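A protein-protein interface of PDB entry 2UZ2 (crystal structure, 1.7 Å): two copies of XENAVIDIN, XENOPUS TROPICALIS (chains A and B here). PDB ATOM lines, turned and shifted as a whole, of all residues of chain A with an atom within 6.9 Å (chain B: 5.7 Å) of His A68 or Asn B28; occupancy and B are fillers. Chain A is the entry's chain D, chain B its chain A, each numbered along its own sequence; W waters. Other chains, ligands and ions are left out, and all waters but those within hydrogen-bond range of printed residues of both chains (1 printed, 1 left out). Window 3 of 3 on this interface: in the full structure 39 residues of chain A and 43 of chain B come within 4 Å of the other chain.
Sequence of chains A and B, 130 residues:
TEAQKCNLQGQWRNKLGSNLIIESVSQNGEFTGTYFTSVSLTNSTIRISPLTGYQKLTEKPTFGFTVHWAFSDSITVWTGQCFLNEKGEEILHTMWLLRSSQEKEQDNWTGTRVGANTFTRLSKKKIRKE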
ATOM      1  N   ILE A  48      -0.813  -7.495 -17.281  1.00  0.00           N
ATOM      2  CA  ILE A  48      -2.103  -7.879 -16.709  1.00  0.00           C
ATOM      3  C   ILE A  48      -1.851  -8.288 -15.260  1.00  0.00           C
ATOM      4  O   ILE A  48      -0.860  -9.014 -14.981  1.00  0.00           O
ATOM      5  CB  ILE A  48      -2.689  -9.066 -17.488  1.00  0.00           C
ATOM      6  CG1 ILE A  48      -2.904  -8.684 -18.956  1.00  0.00           C
ATOM      7  CG2 ILE A  48      -3.978  -9.523 -16.854  1.00  0.00           C
ATOM      8  CD1 ILE A  48      -3.379  -9.824 -19.840  1.00  0.00           C
ATOM      9  N   SER A  49      -2.726  -7.822 -14.362  1.00  0.00           N
ATOM     10  CA  SER A  49      -2.584  -8.056 -12.936  1.00  0.00           C
ATOM     11  C   SER A  49      -3.851  -8.641 -12.343  1.00  0.00           C
ATOM     12  O   SER A  49      -4.946  -8.351 -12.811  1.00  0.00           O
ATOM     13  CB  SER A  49      -2.205  -6.724 -12.242  1.00  0.00           C
ATOM     14  OG  SER A  49      -0.946  -6.242 -12.757  1.00  0.00           O
ATOM     15  N   PRO A  50      -3.710  -9.511 -11.335  1.00  0.00           N
ATOM     16  CA  PRO A  50      -4.897 -10.161 -10.787  1.00  0.00           C
ATOM     17  C   PRO A  50      -5.703  -9.294  -9.824  1.00  0.00           C
ATOM     18  O   PRO A  50      -5.161  -8.400  -9.185  1.00  0.00           O
ATOM     19  CB  PRO A  50      -4.304 -11.339 -10.028  1.00  0.00           C
ATOM     20  CG  PRO A  50      -2.943 -10.808  -9.528  1.00  0.00           C
ATOM     21  CD  PRO A  50      -2.462  -9.974 -10.697  1.00  0.00           C
ATOM     22  N   LEU A  51      -6.987  -9.623  -9.668  1.00  0.00           N
ATOM     23  CA  LEU A  51      -7.808  -8.935  -8.690  1.00  0.00           C
ATOM     24  C   LEU A  51      -8.728  -9.914  -7.988  1.00  0.00           C
ATOM     25  O   LEU A  51      -9.053 -10.986  -8.545  1.00  0.00           O
ATOM     26  CB  LEU A  51      -8.661  -7.838  -9.357  1.00  0.00           C
ATOM     27  CG  LEU A  51      -9.768  -8.284 -10.335  1.00  0.00           C
ATOM     28  CD1 LEU A  51     -11.137  -8.475  -9.697  1.00  0.00           C
ATOM     29  CD2 LEU A  51      -9.877  -7.238 -11.424  1.00  0.00           C
ATOM     30  N   THR A  52      -9.155  -9.514  -6.792  1.00  0.00           N
ATOM     31  CA  THR A  52     -10.178 -10.270  -6.024  1.00  0.00           C
ATOM     32  C   THR A  52     -11.093  -9.242  -5.368  1.00  0.00           C
ATOM     33  O   THR A  52     -10.634  -8.149  -4.973  1.00  0.00           O
ATOM     34  CB  THR A  52      -9.558 -11.143  -4.906  1.00  0.00           C
ATOM     35  OG1 THR A  52     -10.555 -12.052  -4.405  1.00  0.00           O
ATOM     36  CG2 THR A  52      -9.055 -10.277  -3.726  1.00  0.00           C
ATOM     37  N   THR A  66      -9.557  -5.434  -5.092  1.00  0.00           N
ATOM     38  CA  THR A  66      -8.138  -5.012  -4.962  1.00  0.00           C
ATOM     39  C   THR A  66      -7.394  -5.553  -6.174  1.00  0.00           C
ATOM     40  O   THR A  66      -7.613  -6.731  -6.535  1.00  0.00           O
ATOM     41  CB  THR A  66      -7.515  -5.673  -3.715  1.00  0.00           C
ATOM     42  OG1 THR A  66      -8.295  -5.372  -2.532  1.00  0.00           O
ATOM     43  CG2 THR A  66      -6.033  -5.270  -3.528  1.00  0.00           C
ATOM     44  N   VAL A  67      -6.493  -4.738  -6.746  1.00  0.00           N
ATOM     45  CA  VAL A  67      -5.618  -5.202  -7.813  1.00  0.00           C
ATOM     46  C   VAL A  67      -4.222  -5.324  -7.250  1.00  0.00           C
ATOM     47  O   VAL A  67      -3.718  -4.403  -6.631  1.00  0.00           O
ATOM     48  CB  VAL A  67      -5.628  -4.267  -9.037  1.00  0.00           C
ATOM     49  CG1 VAL A  67      -4.586  -4.712 -10.061  1.00  0.00           C
ATOM     50  CG2 VAL A  67      -7.010  -4.303  -9.699  1.00  0.00           C
ATOM     51  N   HIS A  68      -3.613  -6.485  -7.449  1.00  0.00           N
ATOM     52  CA  HIS A  68      -2.245  -6.780  -6.988  1.00  0.00           C
ATOM     53  C   HIS A  68      -1.296  -6.586  -8.173  1.00  0.00           C
ATOM     54  O   HIS A  68      -1.005  -7.517  -8.901  1.00  0.00           O
ATOM     55  CB  HIS A  68      -2.264  -8.226  -6.481  1.00  0.00           C
ATOM     56  CG  HIS A  68      -0.966  -8.736  -5.928  1.00  0.00           C
ATOM     57  ND1 HIS A  68       0.083  -7.932  -5.551  1.00  0.00           N
ATOM     58  CD2 HIS A  68      -0.588 -10.005  -5.642  1.00  0.00           C
ATOM     59  CE1 HIS A  68       1.082  -8.689  -5.117  1.00  0.00           C
ATOM     60  NE2 HIS A  68       0.677  -9.950  -5.124  1.00  0.00           N
ATOM     61  N   TRP A  69      -0.829  -5.351  -8.371  1.00  0.00           N
ATOM     62  CA  TRP A  69      -0.079  -5.028  -9.597  1.00  0.00           C
ATOM     63  C   TRP A  69       1.108  -5.966  -9.710  1.00  0.00           C
ATOM     64  O   TRP A  69       1.905  -6.079  -8.769  1.00  0.00           O
ATOM     65  CB  TRP A  69       0.414  -3.570  -9.575  1.00  0.00           C
ATOM     66  CG  TRP A  69      -0.726  -2.610  -9.470  1.00  0.00           C
ATOM     67  CD1 TRP A  69      -1.040  -1.840  -8.387  1.00  0.00           C
ATOM     68  CD2 TRP A  69      -1.724  -2.340 -10.468  1.00  0.00           C
ATOM     69  NE1 TRP A  69      -2.176  -1.091  -8.647  1.00  0.00           N
ATOM     70  CE2 TRP A  69      -2.620  -1.391  -9.918  1.00  0.00           C
ATOM     71  CE3 TRP A  69      -1.949  -2.818 -11.775  1.00  0.00           C
ATOM     72  CZ2 TRP A  69      -3.735  -0.885 -10.630  1.00  0.00           C
ATOM     73  CZ3 TRP A  69      -3.072  -2.332 -12.483  1.00  0.00           C
ATOM     74  CH2 TRP A  69      -3.939  -1.368 -11.914  1.00  0.00           C
ATOM     75  N   ALA A  70       1.260  -6.554 -10.895  1.00  0.00           N
ATOM     76  CA  ALA A  70       2.289  -7.547 -11.142  1.00  0.00           C
ATOM     77  C   ALA A  70       3.661  -6.947 -11.438  1.00  0.00           C
ATOM     78  O   ALA A  70       4.660  -7.677 -11.505  1.00  0.00           O
ATOM     79  CB  ALA A  70       1.829  -8.469 -12.301  1.00  0.00           C
ATOM     80  N   PHE A  71       3.729  -5.622 -11.592  1.00  0.00           N
ATOM     81  CA  PHE A  71       4.907  -4.965 -12.156  1.00  0.00           C
ATOM     82  C   PHE A  71       5.422  -3.832 -11.260  1.00  0.00           C
ATOM     83  O   PHE A  71       6.350  -3.102 -11.631  1.00  0.00           O
ATOM     84  CB  PHE A  71       4.575  -4.453 -13.568  1.00  0.00           C
ATOM     85  CG  PHE A  71       3.382  -3.549 -13.605  1.00  0.00           C
ATOM     86  CD1 PHE A  71       3.519  -2.183 -13.420  1.00  0.00           C
ATOM     87  CD2 PHE A  71       2.114  -4.086 -13.823  1.00  0.00           C
ATOM     88  CE1 PHE A  71       2.418  -1.340 -13.428  1.00  0.00           C
ATOM     89  CE2 PHE A  71       1.000  -3.288 -13.817  1.00  0.00           C
ATOM     90  CZ  PHE A  71       1.121  -1.910 -13.619  1.00  0.00           C
ATOM     91  N   SER A  72       4.821  -3.687 -10.081  1.00  0.00           N
ATOM     92  CA  SER A  72       5.229  -2.633  -9.137  1.00  0.00           C
ATOM     93  C   SER A  72       4.907  -3.063  -7.707  1.00  0.00           C
ATOM     94  O   SER A  72       4.217  -4.086  -7.515  1.00  0.00           O
ATOM     95  CB  SER A  72       4.513  -1.312  -9.453  1.00  0.00           C
ATOM     96  OG  SER A  72       3.219  -1.357  -8.951  1.00  0.00           O
ATOM     97  N   SER A  74       3.061  -1.353  -5.710  1.00  0.00           N
ATOM     98  CA  SER A  74       1.802  -0.661  -5.386  1.00  0.00           C
ATOM     99  C   SER A  74       0.602  -1.590  -5.285  1.00  0.00           C
ATOM    100  O   SER A  74       0.653  -2.749  -5.714  1.00  0.00           O
ATOM    101  CB  SER A  74       1.486   0.363  -6.481  1.00  0.00           C
ATOM    102  OG  SER A  74       2.543   1.303  -6.592  1.00  0.00           O
ATOM    103  N   ILE A  75      -0.483  -1.090  -4.701  1.00  0.00           N
ATOM    104  CA  ILE A  75      -1.769  -1.795  -4.642  1.00  0.00           C
ATOM    105  C   ILE A  75      -2.822  -0.738  -4.933  1.00  0.00           C
ATOM    106  O   ILE A  75      -2.624   0.437  -4.607  1.00  0.00           O
ATOM    107  CB  ILE A  75      -2.043  -2.357  -3.220  1.00  0.00           C
ATOM    108  CG1 ILE A  75      -1.094  -3.525  -2.847  1.00  0.00           C
ATOM    109  CG2 ILE A  75      -3.530  -2.724  -3.086  1.00  0.00           C
ATOM    110  CD1 ILE A  75      -1.363  -4.851  -3.587  1.00  0.00           C
ATOM    111  N   THR A  76      -3.890  -1.117  -5.624  1.00  0.00           N
ATOM    112  CA  THR A  76      -5.027  -0.193  -5.780  1.00  0.00           C
ATOM    113  C   THR A  76      -6.303  -0.917  -5.401  1.00  0.00           C
ATOM    114  O   THR A  76      -6.455  -2.106  -5.722  1.00  0.00           O
ATOM    115  CB  THR A  76      -5.154   0.330  -7.211  1.00  0.00           C
ATOM    116  OG1 THR A  76      -3.906   0.922  -7.601  1.00  0.00           O
ATOM    117  CG2 THR A  76      -6.294   1.374  -7.330  1.00  0.00           C
ATOM    118  N   SER B  26      -1.065 -16.536   0.954  1.00  0.00           N
ATOM    119  CA  SER B  26      -0.689 -17.481  -0.099  1.00  0.00           C
ATOM    120  C   SER B  26       0.614 -17.101  -0.798  1.00  0.00           C
ATOM    121  O   SER B  26       1.126 -15.985  -0.619  1.00  0.00           O
ATOM    122  CB  SER B  26      -1.819 -17.595  -1.114  1.00  0.00           C
ATOM    123  OG  SER B  26      -2.948 -18.165  -0.492  1.00  0.00           O
ATOM    124  N   GLN B  27       1.150 -18.042  -1.581  1.00  0.00           N
ATOM    125  CA  GLN B  27       2.410 -17.813  -2.340  1.00  0.00           C
ATOM    126  C   GLN B  27       2.407 -16.545  -3.207  1.00  0.00           C
ATOM    127  O   GLN B  27       3.464 -15.915  -3.415  1.00  0.00           O
ATOM    128  CB  GLN B  27       2.763 -19.045  -3.213  1.00  0.00           C
ATOM    129  CG  GLN B  27       1.683 -19.428  -4.260  1.00  0.00           C
ATOM    130  CD  GLN B  27       2.112 -20.542  -5.220  1.00  0.00           C
ATOM    131  OE1 GLN B  27       2.232 -21.722  -4.839  1.00  0.00           O
ATOM    132  NE2 GLN B  27       2.325 -20.175  -6.485  1.00  0.00           N
ATOM    133  N   ASN B  28       1.228 -16.184  -3.711  1.00  0.00           N
ATOM    134  CA  ASN B  28       1.081 -15.040  -4.618  1.00  0.00           C
ATOM    135  C   ASN B  28       0.653 -13.790  -3.876  1.00  0.00           C
ATOM    136  O   ASN B  28       0.297 -12.782  -4.510  1.00  0.00           O
ATOM    137  CB  ASN B  28       0.020 -15.359  -5.666  1.00  0.00           C
ATOM    138  CG  ASN B  28      -1.358 -15.590  -5.050  1.00  0.00           C
ATOM    139  OD1 ASN B  28      -1.508 -15.726  -3.824  1.00  0.00           O
ATOM    140  ND2 ASN B  28      -2.377 -15.632  -5.903  1.00  0.00           N
ATOM    141  N   GLY B  29       0.660 -13.864  -2.546  1.00  0.00           N
ATOM    142  CA  GLY B  29       0.263 -12.719  -1.688  1.00  0.00           C
ATOM    143  C   GLY B  29      -1.216 -12.607  -1.351  1.00  0.00           C
ATOM    144  O   GLY B  29      -1.633 -11.718  -0.597  1.00  0.00           O
ATOM    145  N   GLU B  30      -2.043 -13.508  -1.881  1.00  0.00           N
ATOM    146  CA  GLU B  30      -3.479 -13.431  -1.636  1.00  0.00           C
ATOM    147  C   GLU B  30      -3.786 -13.864  -0.211  1.00  0.00           C
ATOM    148  O   GLU B  30      -3.176 -14.816   0.296  1.00  0.00           O
ATOM    149  CB  GLU B  30      -4.238 -14.330  -2.621  1.00  0.00           C
ATOM    150  CG  GLU B  30      -5.755 -14.263  -2.473  1.00  0.00           C
ATOM    151  CD  GLU B  30      -6.491 -14.933  -3.602  1.00  0.00           C
ATOM    152  OE1 GLU B  30      -6.127 -16.088  -3.958  1.00  0.00           O
ATOM    153  OE2 GLU B  30      -7.456 -14.305  -4.120  1.00  0.00           O
ATOM    154  N   TYR B  54      -4.938  -8.780  -1.055  1.00  0.00           N
ATOM    155  CA  TYR B  54      -3.549  -9.177  -1.352  1.00  0.00           C
ATOM    156  C   TYR B  54      -2.574  -8.327  -0.560  1.00  0.00           C
ATOM    157  O   TYR B  54      -2.822  -7.144  -0.268  1.00  0.00           O
ATOM    158  CB  TYR B  54      -3.191  -8.863  -2.794  1.00  0.00           C
ATOM    159  CG  TYR B  54      -3.956  -9.585  -3.843  1.00  0.00           C
ATOM    160  CD1 TYR B  54      -3.561 -10.846  -4.274  1.00  0.00           C
ATOM    161  CD2 TYR B  54      -5.052  -8.969  -4.432  1.00  0.00           C
ATOM    162  CE1 TYR B  54      -4.275 -11.501  -5.293  1.00  0.00           C
ATOM    163  CE2 TYR B  54      -5.758  -9.592  -5.402  1.00  0.00           C
ATOM    164  CZ  TYR B  54      -5.379 -10.800  -5.841  1.00  0.00           C
ATOM    165  OH  TYR B  54      -6.135 -11.365  -6.828  1.00  0.00           O
ATOM    166  N   GLN B  55      -1.428  -8.931  -0.275  1.00  0.00           N
ATOM    167  CA  GLN B  55      -0.293  -8.198   0.213  1.00  0.00           C
ATOM    168  C   GLN B  55       0.911  -8.392  -0.704  1.00  0.00           C
ATOM    169  O   GLN B  55       1.083  -9.430  -1.323  1.00  0.00           O
ATOM    170  CB  GLN B  55       0.053  -8.613   1.647  1.00  0.00           C
ATOM    171  CG  GLN B  55       0.730  -9.983   1.845  1.00  0.00           C
ATOM    172  CD  GLN B  55       1.515  -9.972   3.150  1.00  0.00           C
ATOM    173  OE1 GLN B  55       1.015 -10.428   4.159  1.00  0.00           O
ATOM    174  NE2 GLN B  55       2.716  -9.360   3.148  1.00  0.00           N
ATOM    175  N   LYS B  56       1.772  -7.378  -0.769  1.00  0.00           N
ATOM    176  CA  LYS B  56       3.066  -7.545  -1.394  1.00  0.00           C
ATOM    177  C   LYS B  56       3.997  -8.447  -0.580  1.00  0.00           C
ATOM    178  O   LYS B  56       3.815  -8.617   0.623  1.00  0.00           O
ATOM    179  CB  LYS B  56       3.728  -6.160  -1.561  1.00  0.00           C
ATOM    180  CG  LYS B  56       3.866  -5.696  -3.007  1.00  0.00           C
ATOM    181  CD  LYS B  56       2.531  -5.520  -3.724  1.00  0.00           C
ATOM    182  CE  LYS B  56       2.760  -5.614  -5.255  1.00  0.00           C
ATOM    183  NZ  LYS B  56       1.500  -5.419  -6.102  1.00  0.00           N
ATOM    184  N   LEU B  57       5.006  -8.991  -1.253  1.00  0.00           N
ATOM    185  CA  LEU B  57       5.896 -10.000  -0.662  1.00  0.00           C
ATOM    186  C   LEU B  57       7.214  -9.372  -0.235  1.00  0.00           C
ATOM    187  O   LEU B  57       8.191 -10.059   0.016  1.00  0.00           O
ATOM    188  CB  LEU B  57       6.153 -11.113  -1.677  1.00  0.00           C
ATOM    189  CG  LEU B  57       4.899 -11.858  -2.148  1.00  0.00           C
ATOM    190  CD1 LEU B  57       5.281 -13.095  -3.007  1.00  0.00           C
ATOM    191  CD2 LEU B  57       4.095 -12.282  -0.919  1.00  0.00           C
HETATM  192  O   HOH W   1       0.474 -12.304  -7.686  1.00  0.00           O
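No position is printed for both chains.
Of the 13 pairs that touch across the chains among the printed residues, none has its exchanged pair printed and touching as well.
Water W1 lies within hydrogen-bond range of O of Asn B28 (3.2 Å) and NE2 of His A68 (3.5 Å).
Hydrophobic or aromatic side chains of chain A within 4 Å of the printed part of chain B: Pro A50, His A68 and Ile A75.
Among the printed residues, no Asp or Glu carboxylate lies within 4 Å of a Lys or Arg side-chain nitrogen of the other chain.
The side-chain amino group (NZ) of Lys B56 is in hydrogen-bond range of the backbone carbonyl oxygen (O) of Ser A74 (2.8 Å).
The backbone carbonyl oxygen of Trp A69 is in hydrogen-bond range of the side-chain amino group of Lys B56 (2.8 Å).
The side-chain hydroxyl of Tyr B54 sits close to the backbone carbonyl oxygen of Leu A51, 3.4 Å away.
The side-chain amino group (NZ) of Lys B56 is in hydrogen-bond range of a ring nitrogen (ND1) of His A68.
The side-chain amino group (NZ) of Lys B56 sits close to the backbone carbonyl oxygen (O) of Ser A72.
O of Asn B28 lies within hydrogen-bond range of NE2 of His A68, at 2.9 Å.
O of Thr A52 is in hydrogen-bond range of N of Thr A66, at 2.9 Å.
The backbone carbonyl oxygen (O) of Pro A50 sits at hydrogen-bond distance from the backbone NH (N) of His A68 (3.0 Å).
The backbone carbonyl oxygen (O) of Gly B29 sits at hydrogen-bond distance from the backbone NH (N) of Gln B55 (2.8 Å).
OG of Ser A72 sits close to N of Ser A74, 3.2 Å away.
The side-chain amide oxygen (OD1) of Asn B28 is in hydrogen-bond range of the backbone NH (N) of Glu B30, at 3.0 Å.
OG of Ser B26 lies close to O of Glu B30 (3.4 Å).
Among the printed residues, merely in contact across the chains: Pro A50 with Tyr B54 (3.7 Å), Thr A52 with Glu B30 (3.8 Å), Thr A52 with Tyr B54 (3.5 Å), Thr A66 with Tyr B54 (3.6 Å), His A68 with Tyr B54 (3.4 Å), His A68 with Gln B55 (3.9 Å) and Ile A75 with Lys B56 (3.9 Å).
Of chain B, only Asn B28 (2.9 Å), Tyr B54 (3.4 Å), Gln B55 (3.9 Å) and Lys B56 (2.9 Å) come within 4 Å of His A68.
Of the printed residues of chain A, Asn B28 touches His A68.
Of the printed residues of chain B, Leu A51 touches Tyr B54.
Of the printed residues of chain A, Tyr B54 touches Pro A50, Leu A51, Thr A52, Thr A66 and His A68.
Of the printed residues of chain A, Lys B56 touches His A68, Trp A69, Ser A72, Ser A74 and Ile A75.
Printed residues of chain B within 4 Å of Thr A66: Tyr B54 (3.6 Å).
The nearest residue of chain A that does not touch Asn B28 is Pro A50 (6.1 Å).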
